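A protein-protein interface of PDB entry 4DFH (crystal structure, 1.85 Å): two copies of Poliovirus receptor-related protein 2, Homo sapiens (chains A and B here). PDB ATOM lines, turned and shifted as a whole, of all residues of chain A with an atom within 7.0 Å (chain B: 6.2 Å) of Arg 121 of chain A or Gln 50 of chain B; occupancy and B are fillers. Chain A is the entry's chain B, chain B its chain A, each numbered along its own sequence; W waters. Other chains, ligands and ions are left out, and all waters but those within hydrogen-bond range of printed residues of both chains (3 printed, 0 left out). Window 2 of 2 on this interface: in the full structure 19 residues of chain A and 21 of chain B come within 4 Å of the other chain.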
ATOM      1  N   ARG A   5      14.203  10.243  -4.555  1.00  0.00           N
ATOM      2  CA  ARG A   5      14.712   9.342  -3.537  1.00  0.00           C
ATOM      3  C   ARG A   5      16.142   8.928  -3.853  1.00  0.00           C
ATOM      4  O   ARG A   5      16.496   8.906  -4.983  1.00  0.00           O
ATOM      5  CB  ARG A   5      13.851   8.095  -3.452  1.00  0.00           C
ATOM      6  CG  ARG A   5      14.005   7.126  -4.608  1.00  0.00           C
ATOM      7  CD  ARG A   5      13.192   5.829  -4.472  1.00  0.00           C
ATOM      8  NE  ARG A   5      12.955   5.173  -5.765  1.00  0.00           N
ATOM      9  CZ  ARG A   5      12.116   5.611  -6.696  1.00  0.00           C
ATOM     10  NH1 ARG A   5      11.421   6.717  -6.496  1.00  0.00           N
ATOM     11  NH2 ARG A   5      11.976   4.938  -7.836  1.00  0.00           N
ATOM     12  N   VAL A   6      16.909   8.569  -2.838  1.00  0.00           N
ATOM     13  CA  VAL A   6      18.286   8.148  -3.032  1.00  0.00           C
ATOM     14  C   VAL A   6      18.361   6.631  -3.085  1.00  0.00           C
ATOM     15  O   VAL A   6      17.852   5.944  -2.200  1.00  0.00           O
ATOM     16  CB  VAL A   6      19.194   8.663  -1.904  1.00  0.00           C
ATOM     17  CG1 VAL A   6      20.614   8.147  -2.091  1.00  0.00           C
ATOM     18  CG2 VAL A   6      19.169  10.184  -1.855  1.00  0.00           C
ATOM     19  N   GLN A   7      18.992   6.113  -4.132  1.00  0.00           N
ATOM     20  CA  GLN A   7      19.180   4.678  -4.274  1.00  0.00           C
ATOM     21  C   GLN A   7      20.590   4.283  -3.846  1.00  0.00           C
ATOM     22  O   GLN A   7      21.577   4.719  -4.439  1.00  0.00           O
ATOM     23  CB  GLN A   7      18.908   4.239  -5.716  1.00  0.00           C
ATOM     24  CG  GLN A   7      18.972   2.733  -5.929  1.00  0.00           C
ATOM     25  CD  GLN A   7      18.063   2.261  -7.052  1.00  0.00           C
ATOM     26  OE1 GLN A   7      16.869   2.557  -7.064  1.00  0.00           O
ATOM     27  NE2 GLN A   7      18.624   1.515  -7.995  1.00  0.00           N
ATOM     28  N   VAL A   8      20.668   3.473  -2.795  1.00  0.00           N
ATOM     29  CA  VAL A   8      21.935   2.961  -2.287  1.00  0.00           C
ATOM     30  C   VAL A   8      21.735   1.530  -1.806  1.00  0.00           C
ATOM     31  O   VAL A   8      20.605   1.058  -1.703  1.00  0.00           O
ATOM     32  CB  VAL A   8      22.460   3.797  -1.106  1.00  0.00           C
ATOM     33  CG1 VAL A   8      22.790   5.219  -1.548  1.00  0.00           C
ATOM     34  CG2 VAL A   8      21.443   3.806   0.025  1.00  0.00           C
ATOM     35  N   CYS A  24      25.418   4.997  -5.397  1.00  0.00           N
ATOM     36  CA  CYS A  24      24.458   6.012  -4.991  1.00  0.00           C
ATOM     37  C   CYS A  24      24.000   6.845  -6.178  1.00  0.00           C
ATOM     38  O   CYS A  24      24.820   7.396  -6.912  1.00  0.00           O
ATOM     39  CB  CYS A  24      25.046   6.926  -3.918  1.00  0.00           C
ATOM     40  SG  CYS A  24      23.925   8.262  -3.441  1.00  0.00           S
ATOM     41  N   LEU A  26      20.345   9.402  -7.641  1.00  0.00           N
ATOM     42  CA  LEU A  26      19.057  10.014  -7.370  1.00  0.00           C
ATOM     43  C   LEU A  26      18.036   9.589  -8.418  1.00  0.00           C
ATOM     44  O   LEU A  26      18.320   9.616  -9.613  1.00  0.00           O
ATOM     45  CB  LEU A  26      19.201  11.536  -7.367  1.00  0.00           C
ATOM     46  CG  LEU A  26      18.018  12.358  -6.856  1.00  0.00           C
ATOM     47  CD1 LEU A  26      17.791  12.094  -5.378  1.00  0.00           C
ATOM     48  CD2 LEU A  26      18.260  13.839  -7.109  1.00  0.00           C
ATOM     49  N   GLN A  41      29.105  11.537   3.824  1.00  0.00           N
ATOM     50  CA  GLN A  41      29.466  11.763   5.211  1.00  0.00           C
ATOM     51  C   GLN A  41      29.626  10.448   5.979  1.00  0.00           C
ATOM     52  O   GLN A  41      29.007   9.511   5.668  1.00  0.00           O
ATOM     53  CB  GLN A  41      28.393  12.571   5.924  1.00  0.00           C
ATOM     54  CG  GLN A  41      28.259  14.022   5.535  1.00  0.00           C
ATOM     55  CD  GLN A  41      27.492  14.833   6.597  1.00  0.00           C
ATOM     56  OE1 GLN A  41      27.995  15.819   7.145  1.00  0.00           O
ATOM     57  NE2 GLN A  41      26.299  14.384   6.914  1.00  0.00           N
ATOM     58  N   THR A 109      26.960   8.072   4.406  1.00  0.00           N
ATOM     59  CA  THR A 109      25.696   8.668   3.991  1.00  0.00           C
ATOM     60  C   THR A 109      25.861   9.485   2.718  1.00  0.00           C
ATOM     61  O   THR A 109      26.684  10.396   2.651  1.00  0.00           O
ATOM     62  CB  THR A 109      25.099   9.562   5.093  1.00  0.00           C
ATOM     63  OG1 THR A 109      24.792   8.763   6.241  1.00  0.00           O
ATOM     64  CG2 THR A 109      23.828  10.235   4.596  1.00  0.00           C
ATOM     65  N   CYS A 110      25.069   9.144   1.709  1.00  0.00           N
ATOM     66  CA  CYS A 110      25.089   9.852   0.439  1.00  0.00           C
ATOM     67  C   CYS A 110      23.933  10.840   0.393  1.00  0.00           C
ATOM     68  O   CYS A 110      22.774  10.440   0.484  1.00  0.00           O
ATOM     69  CB  CYS A 110      24.970   8.857  -0.716  1.00  0.00           C
ATOM     70  SG  CYS A 110      24.964   9.617  -2.348  1.00  0.00           S
ATOM     71  N   GLU A 111      24.235  12.115   0.220  1.00  0.00           N
ATOM     72  CA  GLU A 111      23.252  13.165   0.220  1.00  0.00           C
ATOM     73  C   GLU A 111      23.229  14.037  -1.043  1.00  0.00           C
ATOM     74  O   GLU A 111      24.225  14.447  -1.497  1.00  0.00           O
ATOM     75  CB  GLU A 111      23.456  14.101   1.409  1.00  0.00           C
ATOM     76  CG  GLU A 111      22.343  15.129   1.506  1.00  0.00           C
ATOM     77  CD  GLU A 111      22.644  16.270   2.415  1.00  0.00           C
ATOM     78  OE1 GLU A 111      22.531  17.442   1.988  1.00  0.00           O
ATOM     79  OE2 GLU A 111      22.989  15.933   3.573  1.00  0.00           O
ATOM     80  N   PHE A 112      22.033  14.275  -1.554  1.00  0.00           N
ATOM     81  CA  PHE A 112      21.850  15.204  -2.656  1.00  0.00           C
ATOM     82  C   PHE A 112      21.181  16.458  -2.113  1.00  0.00           C
ATOM     83  O   PHE A 112      20.083  16.388  -1.558  1.00  0.00           O
ATOM     84  CB  PHE A 112      20.961  14.592  -3.742  1.00  0.00           C
ATOM     85  CG  PHE A 112      21.590  13.438  -4.467  1.00  0.00           C
ATOM     86  CD1 PHE A 112      22.221  13.629  -5.685  1.00  0.00           C
ATOM     87  CD2 PHE A 112      21.552  12.161  -3.929  1.00  0.00           C
ATOM     88  CE1 PHE A 112      22.802  12.568  -6.354  1.00  0.00           C
ATOM     89  CE2 PHE A 112      22.134  11.097  -4.591  1.00  0.00           C
ATOM     90  CZ  PHE A 112      22.758  11.302  -5.806  1.00  0.00           C
ATOM     91  N   SER A 119      17.168  18.564   0.721  1.00  0.00           N
ATOM     92  CA  SER A 119      18.174  17.525   0.923  1.00  0.00           C
ATOM     93  C   SER A 119      17.578  16.129   1.106  1.00  0.00           C
ATOM     94  O   SER A 119      16.678  15.926   1.919  1.00  0.00           O
ATOM     95  CB  SER A 119      19.065  17.879   2.119  1.00  0.00           C
ATOM     96  OG  SER A 119      19.871  16.778   2.498  1.00  0.00           O
ATOM     97  N   VAL A 120      18.138  15.153   0.373  1.00  0.00           N
ATOM     98  CA  VAL A 120      17.684  13.782   0.423  1.00  0.00           C
ATOM     99  C   VAL A 120      18.882  12.840   0.558  1.00  0.00           C
ATOM    100  O   VAL A 120      19.879  13.048  -0.049  1.00  0.00           O
ATOM    101  CB  VAL A 120      16.771  13.384  -0.769  1.00  0.00           C
ATOM    102  CG1 VAL A 120      15.536  14.171  -0.763  1.00  0.00           C
ATOM    103  CG2 VAL A 120      17.454  13.586  -2.018  1.00  0.00           C
ATOM    104  N   ARG A 121      18.746  11.787   1.318  1.00  0.00           N
ATOM    105  CA  ARG A 121      19.900  10.958   1.609  1.00  0.00           C
ATOM    106  C   ARG A 121      19.615   9.460   1.646  1.00  0.00           C
ATOM    107  O   ARG A 121      18.507   9.075   1.729  1.00  0.00           O
ATOM    108  CB  ARG A 121      20.546  11.386   2.909  1.00  0.00           C
ATOM    109  CG  ARG A 121      19.911  10.886   4.076  1.00  0.00           C
ATOM    110  CD  ARG A 121      20.268  11.647   5.321  1.00  0.00           C
ATOM    111  NE  ARG A 121      19.989  13.043   5.209  1.00  0.00           N
ATOM    112  CZ  ARG A 121      18.824  13.622   5.480  1.00  0.00           C
ATOM    113  NH1 ARG A 121      17.788  12.933   5.897  1.00  0.00           N
ATOM    114  NH2 ARG A 121      18.727  14.923   5.335  1.00  0.00           N
ATOM    115  N   GLY A 122      20.676   8.669   1.601  1.00  0.00           N
ATOM    116  CA  GLY A 122      20.618   7.233   1.807  1.00  0.00           C
ATOM    117  C   GLY A 122      21.894   6.784   2.494  1.00  0.00           C
ATOM    118  O   GLY A 122      22.968   7.321   2.225  1.00  0.00           O
ATOM    119  N   MET A 123      21.788   5.807   3.388  1.00  0.00           N
ATOM    120  CA  MET A 123      22.950   5.377   4.155  1.00  0.00           C
ATOM    121  C   MET A 123      23.344   3.943   3.825  1.00  0.00           C
ATOM    122  O   MET A 123      22.488   3.087   3.601  1.00  0.00           O
ATOM    123  CB  MET A 123      22.703   5.537   5.658  1.00  0.00           C
ATOM    124  CG  MET A 123      23.953   5.365   6.512  1.00  0.00           C
ATOM    125  SD  MET A 123      23.738   5.908   8.221  1.00  0.00           S
ATOM    126  CE  MET A 123      22.475   4.774   8.793  1.00  0.00           C
ATOM    127  N   TRP B  40      16.244  23.723   5.694  1.00  0.00           N
ATOM    128  CA  TRP B  40      15.732  23.517   7.036  1.00  0.00           C
ATOM    129  C   TRP B  40      15.007  22.185   7.027  1.00  0.00           C
ATOM    130  O   TRP B  40      14.179  21.931   6.151  1.00  0.00           O
ATOM    131  CB  TRP B  40      14.770  24.639   7.430  1.00  0.00           C
ATOM    132  CG  TRP B  40      15.454  25.881   7.929  1.00  0.00           C
ATOM    133  CD1 TRP B  40      15.821  26.968   7.188  1.00  0.00           C
ATOM    134  CD2 TRP B  40      15.840  26.166   9.279  1.00  0.00           C
ATOM    135  NE1 TRP B  40      16.419  27.910   7.993  1.00  0.00           N
ATOM    136  CE2 TRP B  40      16.441  27.443   9.286  1.00  0.00           C
ATOM    137  CE3 TRP B  40      15.742  25.466  10.489  1.00  0.00           C
ATOM    138  CZ2 TRP B  40      16.940  28.035  10.443  1.00  0.00           C
ATOM    139  CZ3 TRP B  40      16.236  26.054  11.642  1.00  0.00           C
ATOM    140  CH2 TRP B  40      16.828  27.324  11.610  1.00  0.00           C
ATOM    141  N   GLN B  41      15.315  21.325   7.976  1.00  0.00           N
ATOM    142  CA  GLN B  41      14.728  20.024   8.049  1.00  0.00           C
ATOM    143  C   GLN B  41      14.176  19.723   9.430  1.00  0.00           C
ATOM    144  O   GLN B  41      14.700  20.153  10.368  1.00  0.00           O
ATOM    145  CB  GLN B  41      15.749  18.955   7.686  1.00  0.00           C
ATOM    146  CG  GLN B  41      16.104  18.837   6.201  1.00  0.00           C
ATOM    147  CD  GLN B  41      16.591  17.448   5.799  1.00  0.00           C
ATOM    148  OE1 GLN B  41      16.971  16.693   6.616  1.00  0.00           O
ATOM    149  NE2 GLN B  41      16.577  17.144   4.513  1.00  0.00           N
ATOM    150  N   ARG B  42      13.124  18.918   9.503  1.00  0.00           N
ATOM    151  CA  ARG B  42      12.654  18.362  10.764  1.00  0.00           C
ATOM    152  C   ARG B  42      13.054  16.890  10.789  1.00  0.00           C
ATOM    153  O   ARG B  42      12.381  16.047  10.195  1.00  0.00           O
ATOM    154  CB  ARG B  42      11.142  18.535  10.907  1.00  0.00           C
ATOM    155  CG  ARG B  42      10.700  19.995  10.923  1.00  0.00           C
ATOM    156  CD  ARG B  42       9.190  20.129  10.981  1.00  0.00           C
ATOM    157  NE  ARG B  42       8.665  19.835  12.309  1.00  0.00           N
ATOM    158  CZ  ARG B  42       7.375  19.879  12.629  1.00  0.00           C
ATOM    159  NH1 ARG B  42       6.471  20.203  11.714  1.00  0.00           N
ATOM    160  NH2 ARG B  42       6.989  19.600  13.866  1.00  0.00           N
ATOM    161  N   PRO B  43      14.170  16.585  11.464  1.00  0.00           N
ATOM    162  CA  PRO B  43      14.799  15.258  11.414  1.00  0.00           C
ATOM    163  C   PRO B  43      13.868  14.154  11.896  1.00  0.00           C
ATOM    164  O   PRO B  43      14.006  13.004  11.476  1.00  0.00           O
ATOM    165  CB  PRO B  43      15.987  15.394  12.374  1.00  0.00           C
ATOM    166  CG  PRO B  43      16.216  16.859  12.516  1.00  0.00           C
ATOM    167  CD  PRO B  43      14.878  17.500  12.374  1.00  0.00           C
ATOM    168  N   ASP B  44      12.925  14.505  12.763  1.00  0.00           N
ATOM    169  CA  ASP B  44      12.033  13.522  13.360  1.00  0.00           C
ATOM    170  C   ASP B  44      10.722  13.369  12.588  1.00  0.00           C
ATOM    171  O   ASP B  44       9.829  12.631  13.005  1.00  0.00           O
ATOM    172  CB  ASP B  44      11.765  13.878  14.821  1.00  0.00           C
ATOM    173  CG  ASP B  44      13.043  13.976  15.636  1.00  0.00           C
ATOM    174  OD1 ASP B  44      14.025  13.283  15.288  1.00  0.00           O
ATOM    175  OD2 ASP B  44      13.069  14.747  16.618  1.00  0.00           O
ATOM    176  N   ALA B  45      10.607  14.069  11.465  1.00  0.00           N
ATOM    177  CA  ALA B  45       9.443  13.923  10.600  1.00  0.00           C
ATOM    178  C   ALA B  45       9.713  12.854   9.544  1.00  0.00           C
ATOM    179  O   ALA B  45      10.868  12.580   9.222  1.00  0.00           O
ATOM    180  CB  ALA B  45       9.107  15.255   9.937  1.00  0.00           C
ATOM    181  N   PRO B  46       8.649  12.244   9.002  1.00  0.00           N
ATOM    182  CA  PRO B  46       8.818  11.277   7.912  1.00  0.00           C
ATOM    183  C   PRO B  46       9.371  11.987   6.681  1.00  0.00           C
ATOM    184  O   PRO B  46       9.247  13.208   6.576  1.00  0.00           O
ATOM    185  CB  PRO B  46       7.382  10.803   7.651  1.00  0.00           C
ATOM    186  CG  PRO B  46       6.536  11.947   8.119  1.00  0.00           C
ATOM    187  CD  PRO B  46       7.233  12.396   9.371  1.00  0.00           C
ATOM    188  N   ALA B  47       9.964  11.232   5.761  1.00  0.00           N
ATOM    189  CA  ALA B  47      10.614  11.811   4.586  1.00  0.00           C
ATOM    190  C   ALA B  47       9.744  12.835   3.857  1.00  0.00           C
ATOM    191  O   ALA B  47      10.244  13.858   3.385  1.00  0.00           O
ATOM    192  CB  ALA B  47      11.056  10.708   3.628  1.00  0.00           C
ATOM    193  N   ASN B  48       8.445  12.559   3.773  1.00  0.00           N
ATOM    194  CA  ASN B  48       7.527  13.421   3.030  1.00  0.00           C
ATOM    195  C   ASN B  48       7.269  14.775   3.685  1.00  0.00           C
ATOM    196  O   ASN B  48       6.711  15.677   3.055  1.00  0.00           O
ATOM    197  CB  ASN B  48       6.193  12.708   2.772  1.00  0.00           C
ATOM    198  CG  ASN B  48       5.546  12.201   4.046  1.00  0.00           C
ATOM    199  OD1 ASN B  48       6.176  11.499   4.837  1.00  0.00           O
ATOM    200  ND2 ASN B  48       4.279  12.542   4.246  1.00  0.00           N
ATOM    201  N   HIS B  49       7.665  14.915   4.947  1.00  0.00           N
ATOM    202  CA  HIS B  49       7.452  16.161   5.677  1.00  0.00           C
ATOM    203  C   HIS B  49       8.756  16.726   6.239  1.00  0.00           C
ATOM    204  O   HIS B  49       8.746  17.682   7.015  1.00  0.00           O
ATOM    205  CB  HIS B  49       6.455  15.957   6.824  1.00  0.00           C
ATOM    206  CG  HIS B  49       5.050  15.691   6.372  1.00  0.00           C
ATOM    207  ND1 HIS B  49       4.140  15.001   7.141  1.00  0.00           N
ATOM    208  CD2 HIS B  49       4.406  16.020   5.228  1.00  0.00           C
ATOM    209  CE1 HIS B  49       2.991  14.921   6.493  1.00  0.00           C
ATOM    210  NE2 HIS B  49       3.125  15.531   5.330  1.00  0.00           N
ATOM    211  N   GLN B  50       9.878  16.141   5.837  1.00  0.00           N
ATOM    212  CA  GLN B  50      11.162  16.460   6.452  1.00  0.00           C
ATOM    213  C   GLN B  50      11.767  17.781   5.979  1.00  0.00           C
ATOM    214  O   GLN B  50      12.274  18.561   6.785  1.00  0.00           O
ATOM    215  CB  GLN B  50      12.148  15.312   6.232  1.00  0.00           C
ATOM    216  CG  GLN B  50      13.414  15.434   7.052  1.00  0.00           C
ATOM    217  CD  GLN B  50      14.152  14.118   7.166  1.00  0.00           C
ATOM    218  OE1 GLN B  50      14.795  13.667   6.218  1.00  0.00           O
ATOM    219  NE2 GLN B  50      14.065  13.493   8.334  1.00  0.00           N
ATOM    220  N   ASN B  51      11.719  18.028   4.673  1.00  0.00           N
ATOM    221  CA  ASN B  51      12.273  19.255   4.104  1.00  0.00           C
ATOM    222  C   ASN B  51      11.263  20.393   4.154  1.00  0.00           C
ATOM    223  O   ASN B  51      10.423  20.520   3.266  1.00  0.00           O
ATOM    224  CB  ASN B  51      12.717  19.028   2.656  1.00  0.00           C
ATOM    225  CG  ASN B  51      14.037  18.291   2.558  1.00  0.00           C
ATOM    226  OD1 ASN B  51      14.081  17.117   2.192  1.00  0.00           O
ATOM    227  ND2 ASN B  51      15.123  18.979   2.884  1.00  0.00           N
ATOM    228  N   VAL B  52      11.344  21.219   5.191  1.00  0.00           N
ATOM    229  CA  VAL B  52      10.353  22.275   5.381  1.00  0.00           C
ATOM    230  C   VAL B  52      10.678  23.536   4.588  1.00  0.00           C
ATOM    231  O   VAL B  52       9.774  24.289   4.216  1.00  0.00           O
ATOM    232  CB  VAL B  52      10.145  22.623   6.873  1.00  0.00           C
ATOM    233  CG1 VAL B  52       9.616  21.409   7.632  1.00  0.00           C
ATOM    234  CG2 VAL B  52      11.436  23.137   7.494  1.00  0.00           C
ATOM    235  N   ALA B  53      11.962  23.764   4.330  1.00  0.00           N
ATOM    236  CA  ALA B  53      12.387  24.935   3.571  1.00  0.00           C
ATOM    237  C   ALA B  53      13.764  24.748   2.935  1.00  0.00           C
ATOM    238  O   ALA B  53      14.618  24.041   3.466  1.00  0.00           O
ATOM    239  CB  ALA B  53      12.365  26.187   4.453  1.00  0.00           C
ATOM    240  N   SER B  65       7.909  20.499   1.903  1.00  0.00           N
ATOM    241  CA  SER B  65       6.892  19.846   2.718  1.00  0.00           C
ATOM    242  C   SER B  65       5.619  20.684   2.809  1.00  0.00           C
ATOM    243  O   SER B  65       5.685  21.906   2.945  1.00  0.00           O
ATOM    244  CB  SER B  65       7.430  19.572   4.120  1.00  0.00           C
ATOM    245  OG  SER B  65       6.405  19.062   4.951  1.00  0.00           O
ATOM    246  N   GLU B 111      20.816  23.598   7.734  1.00  0.00           N
ATOM    247  CA  GLU B 111      21.972  23.048   7.037  1.00  0.00           C
ATOM    248  C   GLU B 111      22.469  23.938   5.908  1.00  0.00           C
ATOM    249  O   GLU B 111      21.689  24.412   5.080  1.00  0.00           O
ATOM    250  CB  GLU B 111      21.656  21.660   6.478  1.00  0.00           C
ATOM    251  CG  GLU B 111      22.731  21.138   5.534  1.00  0.00           C
ATOM    252  CD  GLU B 111      22.298  19.906   4.761  1.00  0.00           C
ATOM    253  OE1 GLU B 111      22.701  19.770   3.586  1.00  0.00           O
ATOM    254  OE2 GLU B 111      21.555  19.075   5.324  1.00  0.00           O
HETATM  255  O   HOH W   1      14.871  13.937   3.593  1.00  0.00           O
HETATM  256  O   HOH W   2      23.898  16.613   6.117  1.00  0.00           O
HETATM  257  O   HOH W   3      20.861  16.690   5.611  1.00  0.00           O
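Among the printed residues, no Asp or Glu carboxylate lies within 4 Å of a Lys or Arg side-chain nitrogen of the other chain.
Glu 111 of chain B touches its own counterpart, Glu 111 of chain A. Of the 5 pairs that touch across the chains among the printed residues, 1 has its exchanged pair printed and touching as well.
The backbone carbonyl oxygen of Asn 51 of chain B lies within hydrogen-bond range of the backbone NH of Ser 65 of chain B, 2.9 Å away. O of Pro 43 of chain B sits at hydrogen-bond distance from NE2 of Gln 50 of chain B. The backbone carbonyl oxygen of Ala 45 of chain B is in hydrogen-bond range of the side-chain amide nitrogen of Gln 50 of chain B (3.4 Å). The backbone NH (N) of Arg 42 of chain B is in hydrogen-bond range of the backbone carbonyl oxygen (O) of Gln 50 of chain B. The side-chain amide nitrogen (NE2) of Gln 41 of chain B lies close to the side-chain amide nitrogen (ND2) of Asn 51 of chain B, at 2.9 Å. The side-chain carboxylate (OE1) of Glu 111 of chain A lies within hydrogen-bond range of the side-chain hydroxyl (OG) of Ser 119 of chain A.
Water W3 lies within hydrogen-bond range of OE2 of Glu 111 of chain B (2.5 Å), NH2 of Arg 121 of chain A (2.8 Å), OE2 of Glu 111 of chain A (3.0 Å) and OG of Ser 119 of chain A (3.3 Å). Water W1 bridges the side-chain amide oxygen (OE1) of Gln 50 of chain B (2.6 Å) and the backbone carbonyl oxygen (O) of Ser 119 of chain A (3.2 Å). Water W2 lies within hydrogen-bond range of OE2 of Glu 111 of chain A (2.8 Å), NE2 of Gln 41 of chain A (3.4 Å) and OE2 of Glu 111 of chain B (3.5 Å).
The side-chain amide oxygen of Asn 51 of chain B sits close to the backbone carbonyl oxygen of Ser 119 of chain A, at 2.9 Å. OE1 of Glu 111 of chain B sits close to OE1 of Glu 111 of chain A, 2.8 Å away. The side-chain amide nitrogen (NE2) of Gln 41 of chain B sits at hydrogen-bond distance from the backbone carbonyl oxygen (O) of Ser 119 of chain A. The side-chain amide oxygen of Gln 41 of chain B sits at hydrogen-bond distance from the guanidinium group of Arg 121 of chain A. NH1 of Arg 121 of chain A lies within hydrogen-bond range of OE1 of Gln 50 of chain B (3.1 Å).
Of the printed residues of chain B, Arg 121 of chain A touches Gln 41 (2.8 Å) and Gln 50 (3.1 Å). Printed residues of chain A within 4 Å of Gln 50 of chain B: Arg 121 (3.1 Å). Of the printed residues of chain B, Ser 119 of chain A touches Gln 41 and Asn 51. Of the printed residues of chain A, Asn 51 of chain B touches Ser 119. Printed residues of chain B within 4 Å of Glu 111 of chain A: Glu 111 (2.8 Å). Printed residues of chain A within 4 Å of Glu 111 of chain B: Glu 111 (2.8 Å). His 49 of chain B touches none of the printed residues of chain A. Leu 26 of chain A touches none of the printed residues of chain B. The nearest residue of chain B that does not touch Arg 121 of chain A is Glu 111 of chain B (5.0 Å). The nearest printed residue of chain B that does not touch Glu 111 of chain A is Gln 41 of chain B (6.5 Å).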
